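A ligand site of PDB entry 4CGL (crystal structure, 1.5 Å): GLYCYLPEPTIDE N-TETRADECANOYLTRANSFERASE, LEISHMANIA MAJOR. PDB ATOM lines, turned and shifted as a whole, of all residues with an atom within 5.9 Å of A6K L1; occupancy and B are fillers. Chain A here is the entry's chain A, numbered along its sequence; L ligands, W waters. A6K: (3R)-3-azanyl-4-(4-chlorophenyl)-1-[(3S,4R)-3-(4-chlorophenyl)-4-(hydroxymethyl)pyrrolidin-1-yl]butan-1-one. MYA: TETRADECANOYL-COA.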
ATOM      1  N   TYR A  70      38.146  -9.298  17.927  1.00  0.00           N
ATOM      2  CA  TYR A  70      36.952  -8.394  18.062  1.00  0.00           C
ATOM      3  C   TYR A  70      37.361  -6.894  18.146  1.00  0.00           C
ATOM      4  O   TYR A  70      38.414  -6.474  17.628  1.00  0.00           O
ATOM      5  CB  TYR A  70      36.083  -8.813  19.227  1.00  0.00           C
ATOM      6  CG  TYR A  70      34.605  -8.345  19.096  1.00  0.00           C
ATOM      7  CD1 TYR A  70      33.912  -8.523  17.836  1.00  0.00           C
ATOM      8  CD2 TYR A  70      33.931  -7.840  20.218  1.00  0.00           C
ATOM      9  CE1 TYR A  70      32.587  -8.125  17.735  1.00  0.00           C
ATOM     10  CE2 TYR A  70      32.581  -7.483  20.161  1.00  0.00           C
ATOM     11  CZ  TYR A  70      31.933  -7.636  18.913  1.00  0.00           C
ATOM     12  OH  TYR A  70      30.653  -7.245  18.957  1.00  0.00           O
ATOM     13  N   VAL A  71      36.432  -6.078  18.605  1.00  0.00           N
ATOM     14  CA  VAL A  71      36.569  -4.640  18.391  1.00  0.00           C
ATOM     15  C   VAL A  71      37.792  -4.095  19.171  1.00  0.00           C
ATOM     16  O   VAL A  71      37.971  -4.396  20.344  1.00  0.00           O
ATOM     17  CB  VAL A  71      35.226  -3.927  18.841  1.00  0.00           C
ATOM     18  CG1 VAL A  71      35.344  -2.351  18.872  1.00  0.00           C
ATOM     19  CG2 VAL A  71      34.051  -4.297  17.908  1.00  0.00           C
ATOM     20  N   PHE A  80      38.465  -5.510  23.150  1.00  0.00           N
ATOM     21  CA  PHE A  80      37.573  -6.110  24.138  1.00  0.00           C
ATOM     22  C   PHE A  80      37.959  -7.556  24.383  1.00  0.00           C
ATOM     23  O   PHE A  80      38.336  -8.246  23.408  1.00  0.00           O
ATOM     24  CB  PHE A  80      36.128  -6.043  23.542  1.00  0.00           C
ATOM     25  CG  PHE A  80      35.480  -4.677  23.677  1.00  0.00           C
ATOM     26  CD1 PHE A  80      35.716  -3.716  22.711  1.00  0.00           C
ATOM     27  CD2 PHE A  80      34.638  -4.432  24.723  1.00  0.00           C
ATOM     28  CE1 PHE A  80      35.135  -2.432  22.816  1.00  0.00           C
ATOM     29  CE2 PHE A  80      34.016  -3.173  24.851  1.00  0.00           C
ATOM     30  CZ  PHE A  80      34.290  -2.199  23.897  1.00  0.00           C
ATOM     31  N   TYR A  82      35.716 -10.079  26.077  1.00  0.00           N
ATOM     32  CA  TYR A  82      34.576 -10.693  26.712  1.00  0.00           C
ATOM     33  C   TYR A  82      34.939 -12.045  27.354  1.00  0.00           C
ATOM     34  O   TYR A  82      35.522 -12.893  26.635  1.00  0.00           O
ATOM     35  CB  TYR A  82      33.495 -10.878  25.603  1.00  0.00           C
ATOM     36  CG  TYR A  82      32.810  -9.623  25.198  1.00  0.00           C
ATOM     37  CD1 TYR A  82      33.346  -8.861  24.128  1.00  0.00           C
ATOM     38  CD2 TYR A  82      31.595  -9.212  25.786  1.00  0.00           C
ATOM     39  CE1 TYR A  82      32.703  -7.652  23.659  1.00  0.00           C
ATOM     40  CE2 TYR A  82      30.950  -8.068  25.307  1.00  0.00           C
ATOM     41  CZ  TYR A  82      31.575  -7.315  24.273  1.00  0.00           C
ATOM     42  OH  TYR A  82      30.860  -6.169  23.924  1.00  0.00           O
ATOM     43  N   PHE A  86      30.625 -14.368  30.426  1.00  0.00           N
ATOM     44  CA  PHE A  86      29.844 -13.285  29.824  1.00  0.00           C
ATOM     45  C   PHE A  86      29.170 -13.733  28.495  1.00  0.00           C
ATOM     46  O   PHE A  86      27.995 -13.436  28.236  1.00  0.00           O
ATOM     47  CB  PHE A  86      30.756 -12.078  29.491  1.00  0.00           C
ATOM     48  CG  PHE A  86      29.993 -10.822  29.147  1.00  0.00           C
ATOM     49  CD1 PHE A  86      29.395 -10.662  27.879  1.00  0.00           C
ATOM     50  CD2 PHE A  86      29.976  -9.724  30.064  1.00  0.00           C
ATOM     51  CE1 PHE A  86      28.662  -9.520  27.556  1.00  0.00           C
ATOM     52  CE2 PHE A  86      29.338  -8.501  29.700  1.00  0.00           C
ATOM     53  CZ  PHE A  86      28.669  -8.376  28.493  1.00  0.00           C
ATOM     54  N   ILE A 156      21.261  -8.646  16.607  1.00  0.00           N
ATOM     55  CA  ILE A 156      22.455  -9.208  16.028  1.00  0.00           C
ATOM     56  C   ILE A 156      23.661  -8.529  16.722  1.00  0.00           C
ATOM     57  O   ILE A 156      23.666  -7.295  16.909  1.00  0.00           O
ATOM     58  CB  ILE A 156      22.560  -8.912  14.489  1.00  0.00           C
ATOM     59  CG1 ILE A 156      21.497  -9.781  13.698  1.00  0.00           C
ATOM     60  CG2 ILE A 156      23.979  -9.201  14.050  1.00  0.00           C
ATOM     61  CD1 ILE A 156      21.834 -11.234  13.589  1.00  0.00           C
ATOM     62  N   ASN A 157      24.646  -9.354  17.100  1.00  0.00           N
ATOM     63  CA  ASN A 157      25.839  -8.773  17.814  1.00  0.00           C
ATOM     64  C   ASN A 157      26.967  -9.740  17.549  1.00  0.00           C
ATOM     65  O   ASN A 157      26.803 -10.817  17.030  1.00  0.00           O
ATOM     66  CB  ASN A 157      25.495  -8.631  19.279  1.00  0.00           C
ATOM     67  CG  ASN A 157      26.352  -7.549  19.999  1.00  0.00           C
ATOM     68  OD1 ASN A 157      27.316  -7.006  19.439  1.00  0.00           O
ATOM     69  ND2 ASN A 157      25.963  -7.245  21.200  1.00  0.00           N
ATOM     70  N   PHE A 158      28.187  -9.354  17.959  1.00  0.00           N
ATOM     71  CA  PHE A 158      29.360 -10.221  17.949  1.00  0.00           C
ATOM     72  C   PHE A 158      29.791 -10.637  16.570  1.00  0.00           C
ATOM     73  O   PHE A 158      30.455 -11.688  16.488  1.00  0.00           O
ATOM     74  CB  PHE A 158      29.240 -11.411  18.950  1.00  0.00           C
ATOM     75  CG  PHE A 158      29.004 -10.951  20.346  1.00  0.00           C
ATOM     76  CD1 PHE A 158      30.072 -10.361  21.081  1.00  0.00           C
ATOM     77  CD2 PHE A 158      27.783 -11.124  20.987  1.00  0.00           C
ATOM     78  CE1 PHE A 158      29.876  -9.931  22.391  1.00  0.00           C
ATOM     79  CE2 PHE A 158      27.552 -10.714  22.313  1.00  0.00           C
ATOM     80  CZ  PHE A 158      28.610 -10.054  23.019  1.00  0.00           C
ATOM     81  N   TYR A 192      20.548  -3.826  15.396  1.00  0.00           N
ATOM     82  CA  TYR A 192      22.016  -4.027  15.601  1.00  0.00           C
ATOM     83  C   TYR A 192      22.643  -2.663  15.801  1.00  0.00           C
ATOM     84  O   TYR A 192      22.113  -1.650  15.338  1.00  0.00           O
ATOM     85  CB  TYR A 192      22.690  -4.758  14.434  1.00  0.00           C
ATOM     86  CG  TYR A 192      22.394  -4.258  13.041  1.00  0.00           C
ATOM     87  CD1 TYR A 192      21.202  -4.573  12.383  1.00  0.00           C
ATOM     88  CD2 TYR A 192      23.324  -3.442  12.354  1.00  0.00           C
ATOM     89  CE1 TYR A 192      20.973  -4.113  11.075  1.00  0.00           C
ATOM     90  CE2 TYR A 192      23.114  -3.036  11.033  1.00  0.00           C
ATOM     91  CZ  TYR A 192      21.925  -3.343  10.397  1.00  0.00           C
ATOM     92  OH  TYR A 192      21.686  -2.834   9.125  1.00  0.00           O
ATOM     93  N   THR A 193      23.774  -2.628  16.504  1.00  0.00           N
ATOM     94  CA  THR A 193      24.520  -1.384  16.579  1.00  0.00           C
ATOM     95  C   THR A 193      25.904  -1.683  15.964  1.00  0.00           C
ATOM     96  O   THR A 193      26.400  -2.781  15.902  1.00  0.00           O
ATOM     97  CB  THR A 193      24.709  -0.932  18.018  1.00  0.00           C
ATOM     98  OG1 THR A 193      25.109  -2.054  18.835  1.00  0.00           O
ATOM     99  CG2 THR A 193      23.466  -0.292  18.597  1.00  0.00           C
ATOM    100  N   ALA A 194      26.598  -0.597  15.605  1.00  0.00           N
ATOM    101  CA  ALA A 194      28.015  -0.669  15.188  1.00  0.00           C
ATOM    102  C   ALA A 194      28.635   0.709  15.510  1.00  0.00           C
ATOM    103  O   ALA A 194      27.964   1.755  15.476  1.00  0.00           O
ATOM    104  CB  ALA A 194      28.139  -0.969  13.733  1.00  0.00           C
ATOM    105  N   GLY A 195      29.965   0.667  15.678  1.00  0.00           N
ATOM    106  CA  GLY A 195      30.723   1.908  15.915  1.00  0.00           C
ATOM    107  C   GLY A 195      31.234   2.452  14.600  1.00  0.00           C
ATOM    108  O   GLY A 195      32.157   3.286  14.629  1.00  0.00           O
ATOM    109  N   TYR A 207      29.867   8.214  23.047  1.00  0.00           N
ATOM    110  CA  TYR A 207      30.299   7.397  24.229  1.00  0.00           C
ATOM    111  C   TYR A 207      30.741   8.294  25.361  1.00  0.00           C
ATOM    112  O   TYR A 207      31.259   9.460  25.139  1.00  0.00           O
ATOM    113  CB  TYR A 207      31.436   6.556  23.851  1.00  0.00           C
ATOM    114  CG  TYR A 207      31.246   5.709  22.613  1.00  0.00           C
ATOM    115  CD1 TYR A 207      30.654   4.458  22.757  1.00  0.00           C
ATOM    116  CD2 TYR A 207      31.712   6.061  21.351  1.00  0.00           C
ATOM    117  CE1 TYR A 207      30.553   3.595  21.672  1.00  0.00           C
ATOM    118  CE2 TYR A 207      31.613   5.244  20.218  1.00  0.00           C
ATOM    119  CZ  TYR A 207      31.073   3.955  20.392  1.00  0.00           C
ATOM    120  OH  TYR A 207      30.973   3.101  19.312  1.00  0.00           O
ATOM    121  N   PHE A 208      30.614   7.763  26.555  1.00  0.00           N
ATOM    122  CA  PHE A 208      31.063   8.513  27.757  1.00  0.00           C
ATOM    123  C   PHE A 208      31.810   7.650  28.716  1.00  0.00           C
ATOM    124  O   PHE A 208      31.444   6.483  28.903  1.00  0.00           O
ATOM    125  CB  PHE A 208      29.855   9.182  28.448  1.00  0.00           C
ATOM    126  CG  PHE A 208      29.282  10.290  27.623  1.00  0.00           C
ATOM    127  CD1 PHE A 208      29.776  11.622  27.780  1.00  0.00           C
ATOM    128  CD2 PHE A 208      28.263  10.045  26.734  1.00  0.00           C
ATOM    129  CE1 PHE A 208      29.281  12.652  26.953  1.00  0.00           C
ATOM    130  CE2 PHE A 208      27.784  11.041  25.917  1.00  0.00           C
ATOM    131  CZ  PHE A 208      28.308  12.361  26.035  1.00  0.00           C
ATOM    132  N   HIS A 209      32.816   8.224  29.412  1.00  0.00           N
ATOM    133  CA  HIS A 209      33.652   7.422  30.343  1.00  0.00           C
ATOM    134  C   HIS A 209      33.858   8.216  31.655  1.00  0.00           C
ATOM    135  O   HIS A 209      33.933   9.412  31.659  1.00  0.00           O
ATOM    136  CB  HIS A 209      34.985   7.091  29.658  1.00  0.00           C
ATOM    137  CG  HIS A 209      35.707   8.289  29.167  1.00  0.00           C
ATOM    138  ND1 HIS A 209      36.143   9.290  30.008  1.00  0.00           N
ATOM    139  CD2 HIS A 209      36.038   8.688  27.909  1.00  0.00           C
ATOM    140  CE1 HIS A 209      36.709  10.250  29.300  1.00  0.00           C
ATOM    141  NE2 HIS A 209      36.655   9.913  28.030  1.00  0.00           N
ATOM    142  N   TYR A 316      27.419  -4.018  33.891  1.00  0.00           N
ATOM    143  CA  TYR A 316      28.086  -5.284  33.485  1.00  0.00           C
ATOM    144  C   TYR A 316      29.592  -5.058  33.258  1.00  0.00           C
ATOM    145  O   TYR A 316      30.070  -3.957  33.064  1.00  0.00           O
ATOM    146  CB  TYR A 316      27.403  -6.004  32.287  1.00  0.00           C
ATOM    147  CG  TYR A 316      27.364  -5.125  31.052  1.00  0.00           C
ATOM    148  CD1 TYR A 316      28.478  -5.032  30.169  1.00  0.00           C
ATOM    149  CD2 TYR A 316      26.193  -4.347  30.783  1.00  0.00           C
ATOM    150  CE1 TYR A 316      28.444  -4.234  28.980  1.00  0.00           C
ATOM    151  CE2 TYR A 316      26.172  -3.512  29.645  1.00  0.00           C
ATOM    152  CZ  TYR A 316      27.232  -3.459  28.792  1.00  0.00           C
ATOM    153  OH  TYR A 316      27.248  -2.599  27.719  1.00  0.00           O
ATOM    154  N   ILE A 318      33.236  -5.818  31.320  1.00  0.00           N
ATOM    155  CA  ILE A 318      34.014  -6.394  30.180  1.00  0.00           C
ATOM    156  C   ILE A 318      35.415  -5.893  30.364  1.00  0.00           C
ATOM    157  O   ILE A 318      35.631  -4.678  30.410  1.00  0.00           O
ATOM    158  CB  ILE A 318      33.571  -6.016  28.752  1.00  0.00           C
ATOM    159  CG1 ILE A 318      32.061  -6.189  28.584  1.00  0.00           C
ATOM    160  CG2 ILE A 318      34.301  -6.925  27.714  1.00  0.00           C
ATOM    161  CD1 ILE A 318      31.534  -5.470  27.327  1.00  0.00           C
ATOM    162  N   TYR A 335      30.186  -1.083  32.678  1.00  0.00           N
ATOM    163  CA  TYR A 335      29.294  -0.444  31.657  1.00  0.00           C
ATOM    164  C   TYR A 335      27.921  -0.309  32.260  1.00  0.00           C
ATOM    165  O   TYR A 335      27.350  -1.263  32.801  1.00  0.00           O
ATOM    166  CB  TYR A 335      29.179  -1.413  30.463  1.00  0.00           C
ATOM    167  CG  TYR A 335      30.493  -1.443  29.714  1.00  0.00           C
ATOM    168  CD1 TYR A 335      31.522  -2.309  30.111  1.00  0.00           C
ATOM    169  CD2 TYR A 335      30.687  -0.683  28.586  1.00  0.00           C
ATOM    170  CE1 TYR A 335      32.710  -2.308  29.441  1.00  0.00           C
ATOM    171  CE2 TYR A 335      31.918  -0.642  27.922  1.00  0.00           C
ATOM    172  CZ  TYR A 335      32.940  -1.523  28.378  1.00  0.00           C
ATOM    173  OH  TYR A 335      34.149  -1.470  27.699  1.00  0.00           O
ATOM    174  N   ASN A 366      31.696   3.169  31.877  1.00  0.00           N
ATOM    175  CA  ASN A 366      31.433   3.525  30.475  1.00  0.00           C
ATOM    176  C   ASN A 366      29.928   3.456  30.102  1.00  0.00           C
ATOM    177  O   ASN A 366      29.172   2.676  30.750  1.00  0.00           O
ATOM    178  CB  ASN A 366      32.149   2.503  29.567  1.00  0.00           C
ATOM    179  CG  ASN A 366      33.638   2.650  29.563  1.00  0.00           C
ATOM    180  OD1 ASN A 366      34.170   3.718  29.765  1.00  0.00           O
ATOM    181  ND2 ASN A 366      34.295   1.564  29.180  1.00  0.00           N
ATOM    182  N   MET A 367      29.488   4.288  29.147  1.00  0.00           N
ATOM    183  CA  MET A 367      28.079   4.243  28.745  1.00  0.00           C
ATOM    184  C   MET A 367      27.927   4.999  27.402  1.00  0.00           C
ATOM    185  O   MET A 367      28.837   5.661  26.923  1.00  0.00           O
ATOM    186  CB  MET A 367      27.177   4.892  29.795  1.00  0.00           C
ATOM    187  CG  MET A 367      27.293   6.423  29.873  1.00  0.00           C
ATOM    188  SD  MET A 367      26.397   7.100  31.218  1.00  0.00           S
ATOM    189  CE  MET A 367      26.800   8.923  30.993  1.00  0.00           C
ATOM    190  N   VAL A 368      26.781   4.774  26.767  1.00  0.00           N
ATOM    191  CA  VAL A 368      26.421   5.513  25.530  1.00  0.00           C
ATOM    192  C   VAL A 368      25.304   6.493  25.951  1.00  0.00           C
ATOM    193  O   VAL A 368      24.659   6.295  27.012  1.00  0.00           O
ATOM    194  CB  VAL A 368      26.014   4.559  24.458  1.00  0.00           C
ATOM    195  CG1 VAL A 368      25.585   5.302  23.189  1.00  0.00           C
ATOM    196  CG2 VAL A 368      27.148   3.575  24.128  1.00  0.00           C
ATOM    197  N   LEU A 389      28.318   5.678  18.466  1.00  0.00           N
ATOM    198  CA  LEU A 389      27.634   4.384  18.314  1.00  0.00           C
ATOM    199  C   LEU A 389      26.402   4.635  17.458  1.00  0.00           C
ATOM    200  O   LEU A 389      25.695   5.615  17.790  1.00  0.00           O
ATOM    201  CB  LEU A 389      27.219   3.865  19.722  1.00  0.00           C
ATOM    202  CG  LEU A 389      26.735   2.434  19.530  1.00  0.00           C
ATOM    203  CD1 LEU A 389      27.823   1.458  19.054  1.00  0.00           C
ATOM    204  CD2 LEU A 389      26.104   1.986  20.847  1.00  0.00           C
ATOM    205  N   MET A 410      23.014  -2.581  24.204  1.00  0.00           N
ATOM    206  CA  MET A 410      23.552  -3.646  23.416  1.00  0.00           C
ATOM    207  C   MET A 410      24.890  -4.075  24.040  1.00  0.00           C
ATOM    208  O   MET A 410      25.748  -3.222  24.367  1.00  0.00           O
ATOM    209  CB  MET A 410      23.951  -3.106  22.051  1.00  0.00           C
ATOM    210  CG  MET A 410      22.739  -2.659  21.226  1.00  0.00           C
ATOM    211  SD  MET A 410      22.002  -4.165  20.593  1.00  0.00           S
ATOM    212  CE  MET A 410      21.357  -3.619  19.072  1.00  0.00           C
ATOM    213  N   LEU A 411      25.076  -5.381  24.267  1.00  0.00           N
ATOM    214  CA  LEU A 411      26.191  -5.790  25.173  1.00  0.00           C
ATOM    215  C   LEU A 411      27.459  -5.857  24.343  1.00  0.00           C
ATOM    216  O   LEU A 411      27.536  -6.032  23.085  1.00  0.00           O
ATOM    217  CB  LEU A 411      25.837  -7.207  25.721  1.00  0.00           C
ATOM    218  CG  LEU A 411      24.633  -7.299  26.684  1.00  0.00           C
ATOM    219  CD1 LEU A 411      24.284  -8.731  26.970  1.00  0.00           C
ATOM    220  CD2 LEU A 411      24.810  -6.452  27.924  1.00  0.00           C
ATOM    221  OXT LEU A 411      28.586  -5.798  25.011  1.00  0.00           O
HETATM  222 CL1  A6K L   1      33.131   0.402  21.194  1.00  0.00          CL
HETATM  223  C18 A6K L   1      32.050  -0.837  20.466  1.00  0.00           C
HETATM  224  C17 A6K L   1      32.132  -2.152  20.950  1.00  0.00           C
HETATM  225  C16 A6K L   1      31.265  -3.074  20.316  1.00  0.00           C
HETATM  226  C19 A6K L   1      31.110  -0.426  19.533  1.00  0.00           C
HETATM  227  C20 A6K L   1      30.268  -1.319  18.926  1.00  0.00           C
HETATM  228  C15 A6K L   1      30.359  -2.655  19.315  1.00  0.00           C
HETATM  229  C14 A6K L   1      29.403  -3.674  18.658  1.00  0.00           C
HETATM  230  C   A6K L   1      27.895  -3.438  19.009  1.00  0.00           C
HETATM  231  N   A6K L   1      27.125  -4.416  18.178  1.00  0.00           N
HETATM  232  C1  A6K L   1      27.585  -3.618  20.495  1.00  0.00           C
HETATM  233  C2  A6K L   1      27.662  -2.241  21.155  1.00  0.00           C
HETATM  234  O   A6K L   1      26.949  -1.346  20.657  1.00  0.00           O
HETATM  235  N1  A6K L   1      28.337  -1.934  22.265  1.00  0.00           N
HETATM  236  C7  A6K L   1      28.404  -0.598  22.967  1.00  0.00           C
HETATM  237  C6  A6K L   1      29.122  -0.922  24.297  1.00  0.00           C
HETATM  238  C4  A6K L   1      29.961  -2.144  23.963  1.00  0.00           C
HETATM  239  C5  A6K L   1      30.204  -2.967  25.232  1.00  0.00           C
HETATM  240  O1  A6K L   1      29.030  -3.368  25.933  1.00  0.00           O
HETATM  241  C3  A6K L   1      29.051  -2.945  23.072  1.00  0.00           C
HETATM  242  C8  A6K L   1      29.920   0.272  24.756  1.00  0.00           C
HETATM  243  C13 A6K L   1      31.131   0.641  24.133  1.00  0.00           C
HETATM  244  C12 A6K L   1      31.812   1.767  24.619  1.00  0.00           C
HETATM  245  C11 A6K L   1      31.221   2.446  25.654  1.00  0.00           C
HETATM  246 CL   A6K L   1      32.140   3.853  26.266  1.00  0.00          CL
HETATM  247  C10 A6K L   1      30.040   2.139  26.343  1.00  0.00           C
HETATM  248  C9  A6K L   1      29.371   1.021  25.827  1.00  0.00           C
HETATM  249  S1  MYA L   2      29.222  -4.506  15.029  1.00  0.00           S
HETATM  250  C2  MYA L   2      30.790  -5.228  15.517  1.00  0.00           C
HETATM  251  C3  MYA L   2      31.534  -5.605  14.252  1.00  0.00           C
HETATM  252  N4  MYA L   2      32.813  -6.343  14.589  1.00  0.00           N
HETATM  253  C5  MYA L   2      34.004  -5.719  14.675  1.00  0.00           C
HETATM  254  O5  MYA L   2      34.118  -4.539  14.343  1.00  0.00           O
HETATM  255  C6  MYA L   2      35.140  -6.643  15.018  1.00  0.00           C
HETATM  256  C7  MYA L   2      36.392  -6.375  14.147  1.00  0.00           C
HETATM  257  N8  MYA L   2      36.177  -6.292  12.747  1.00  0.00           N
HETATM  258  C9  MYA L   2      35.848  -7.378  12.033  1.00  0.00           C
HETATM  259  O9  MYA L   2      35.691  -8.453  12.659  1.00  0.00           O
HETATM  260  C10 MYA L   2      35.584  -7.279  10.581  1.00  0.00           C
HETATM  261  O10 MYA L   2      36.220  -6.088  10.095  1.00  0.00           O
HETATM  262  C11 MYA L   2      34.092  -7.161  10.182  1.00  0.00           C
HETATM  263  C12 MYA L   2      33.961  -6.920   8.701  1.00  0.00           C
HETATM  264  C13 MYA L   2      33.341  -6.009  10.907  1.00  0.00           C
HETATM  265  C14 MYA L   2      33.452  -8.521  10.472  1.00  0.00           C
HETATM  266  N1A MYA L   2      28.287  -4.341  10.319  1.00  0.00           N
HETATM  267  O1A MYA L   2      35.075  -7.812   3.151  1.00  0.00           O
HETATM  268  P1A MYA L   2      34.257  -7.925   4.430  1.00  0.00           P
HETATM  269  C1X MYA L   2      30.346  -4.335   5.586  1.00  0.00           C
HETATM  270  C2A MYA L   2      27.816  -4.610   9.127  1.00  0.00           C
HETATM  271  O2A MYA L   2      34.110  -9.279   4.912  1.00  0.00           O
HETATM  272  P2A MYA L   2      35.810  -7.413   6.857  1.00  0.00           P
HETATM  273  C2M MYA L   2      28.102  -5.839  15.115  1.00  0.00           C
HETATM  274  O2M MYA L   2      28.432  -6.911  15.637  1.00  0.00           O
HETATM  275  C2X MYA L   2      31.062  -3.287   4.696  1.00  0.00           C
HETATM  276  O2X MYA L   2      30.384  -2.045   4.714  1.00  0.00           O
HETATM  277  N3A MYA L   2      28.435  -4.540   7.919  1.00  0.00           N
HETATM  278  O3A MYA L   2      34.956  -6.973   5.571  1.00  0.00           O
HETATM  279  C3M MYA L   2      26.713  -5.712  14.441  1.00  0.00           C
HETATM  280  C3X MYA L   2      31.088  -4.075   3.414  1.00  0.00           C
HETATM  281  O3X MYA L   2      29.832  -4.023   2.673  1.00  0.00           O
HETATM  282  P3X MYA L   2      29.656  -3.024   1.407  1.00  0.00           P
HETATM  283  C4A MYA L   2      29.756  -4.256   7.987  1.00  0.00           C
HETATM  284  O4A MYA L   2      36.629  -8.646   6.648  1.00  0.00           O
HETATM  285  C4M MYA L   2      26.826  -6.407  13.102  1.00  0.00           C
HETATM  286  C4X MYA L   2      31.295  -5.477   3.831  1.00  0.00           C
HETATM  287  O4X MYA L   2      30.920  -5.535   5.236  1.00  0.00           O
HETATM  288  C5A MYA L   2      30.351  -3.951   9.198  1.00  0.00           C
HETATM  289  O5A MYA L   2      36.431  -6.094   7.372  1.00  0.00           O
HETATM  290  C5M MYA L   2      25.526  -6.114  12.266  1.00  0.00           C
HETATM  291  C5X MYA L   2      32.773  -5.907   3.711  1.00  0.00           C
HETATM  292  O5X MYA L   2      32.912  -7.239   4.089  1.00  0.00           O
HETATM  293  C6A MYA L   2      29.621  -4.041  10.379  1.00  0.00           C
HETATM  294  N6A MYA L   2      30.164  -3.740  11.568  1.00  0.00           N
HETATM  295  O6A MYA L   2      34.656  -7.888   7.911  1.00  0.00           O
HETATM  296  C6M MYA L   2      25.602  -6.964  10.996  1.00  0.00           C
HETATM  297  N7A MYA L   2      31.692  -3.678   8.961  1.00  0.00           N
HETATM  298  O7A MYA L   2      28.207  -3.139   0.969  1.00  0.00           O
HETATM  299  C7M MYA L   2      24.398  -6.742  10.073  1.00  0.00           C
HETATM  300  C8A MYA L   2      31.830  -3.732   7.608  1.00  0.00           C
HETATM  301  O8A MYA L   2      30.675  -3.572   0.441  1.00  0.00           O
HETATM  302  C8M MYA L   2      23.206  -7.675  10.542  1.00  0.00           C
HETATM  303  N9A MYA L   2      30.638  -4.100   7.008  1.00  0.00           N
HETATM  304  O9A MYA L   2      29.938  -1.677   2.066  1.00  0.00           O
HETATM  305  C9M MYA L   2      21.994  -7.430   9.550  1.00  0.00           C
HETATM  306  CAM MYA L   2      20.760  -8.236  10.070  1.00  0.00           C
HETATM  307  CBM MYA L   2      20.872  -9.725   9.812  1.00  0.00           C
HETATM  308  CCM MYA L   2      19.677 -10.585  10.368  1.00  0.00           C
HETATM  309  CDM MYA L   2      18.404 -10.218   9.633  1.00  0.00           C
HETATM  310  CEM MYA L   2      17.247 -11.101  10.271  1.00  0.00           C
HETATM  311  CFM MYA L   2      15.889 -10.568   9.766  1.00  0.00           C
HETATM  312  O   HOH W   1      25.806  -0.714  25.387  1.00  0.00           O
HETATM  313  O   HOH W   2      34.628   0.993  18.284  1.00  0.00           O
HETATM  314  O   HOH W   3      24.362  -5.068  18.163  1.00  0.00           O
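OXT of Leu 411 lies within hydrogen-bond range of O1 of A6K L1 (2.6 Å). The side-chain hydroxyl of Tyr 316 lies within hydrogen-bond range of an oxygen (O1) of A6K L1 (2.6 Å). A nitrogen (N) of A6K L1 is in hydrogen-bond range of the backbone carbonyl oxygen (O) of Thr 193, 2.9 Å away. The side-chain hydroxyl (OG1) of Thr 193 lies within hydrogen-bond range of an oxygen (O) of A6K L1 (2.7 Å). OD1 of Asn 157 is in hydrogen-bond range of N of A6K L1 (2.9 Å). An oxygen (O2M) of MYA L2 lies within hydrogen-bond range of the backbone NH of Phe 158 (3.4 Å).
A nitrogen (N) of A6K L1 lies close to a sulfur (S1) of MYA L2 (3.8 Å).
O of Leu 411 is in hydrogen-bond range of ND2 of Asn 157, 2.7 Å away. The side-chain hydroxyl (OH) of Tyr 82 is in hydrogen-bond range of the chain-end carboxylate (OXT) of Leu 411, at 2.5 Å. The backbone NH of Tyr 335 sits at hydrogen-bond distance from the backbone carbonyl oxygen of Tyr 316 (2.9 Å). The side-chain amide oxygen of Asn 157 is in hydrogen-bond range of the side-chain hydroxyl of Tyr 70. The side-chain amide nitrogen (ND2) of Asn 366 is in hydrogen-bond range of the side-chain hydroxyl (OH) of Tyr 335 (3.4 Å). The backbone carbonyl oxygen of Val 71 lies within hydrogen-bond range of the backbone NH of Phe 80 (3.1 Å). O of Met 367 sits at hydrogen-bond distance from N of Phe 208 (2.8 Å). The side-chain hydroxyl (OH) of Tyr 70 is in hydrogen-bond range of the backbone NH (N) of Phe 158, at 3.4 Å.
Tyr 70 touches A6K L1 (OH to C14, 3.8 Å). Val 71 touches A6K L1 (CG1 to C17, 3.8 Å). Phe 80 touches A6K L1. Tyr 82 touches A6K L1 (OH to C5, 3.5 Å). Gly 195 touches A6K L1 (N to C20, 3.8 Å). Tyr 207 touches A6K L1 (CD1 to C12, 3.5 Å). Phe 208 touches A6K L1. Ile 318 touches A6K L1 (CD1 to C5, 3.5 Å). Tyr 335 touches A6K L1 (CD2 to C9, 3.5 Å). Asn 366 touches A6K L1 (CB to CL, 3.6 Å). N of Met 367 touches C10 of A6K L1, at 3.6 Å. Val 368 touches A6K L1 (CG2 to C9, 3.8 Å). CD1 of Leu 389 touches O of A6K L1, at 3.3 Å. Met 410 touches A6K L1. Hydrophobic or aromatic side chains that line A6K L1: Val 71, Phe 80, Tyr 207, Tyr 316, Ile 318, Tyr 335, Val 368, Leu 389 and Met 410. Within 4 Å of A6K L1: Tyr 70, Val 71, Phe 80, Tyr 82, Asn 157, Thr 193, Gly 195, Tyr 207, Phe 208, Tyr 316, Ile 318, Tyr 335, Asn 366, Met 367, Val 368, Leu 389, Met 410 and Leu 411.
Water W3 lies within hydrogen-bond range of the backbone carbonyl oxygen (O) of Ile 156 (2.6 Å), a nitrogen (N) of A6K L1 (2.8 Å), the backbone NH (N) of Thr 193 (3.0 Å) and the side-chain sulfur (SD) of Met 410 (3.5 Å). Water W1 bridges O of Met 410 (2.7 Å) and OH of Tyr 316 (3.3 Å).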
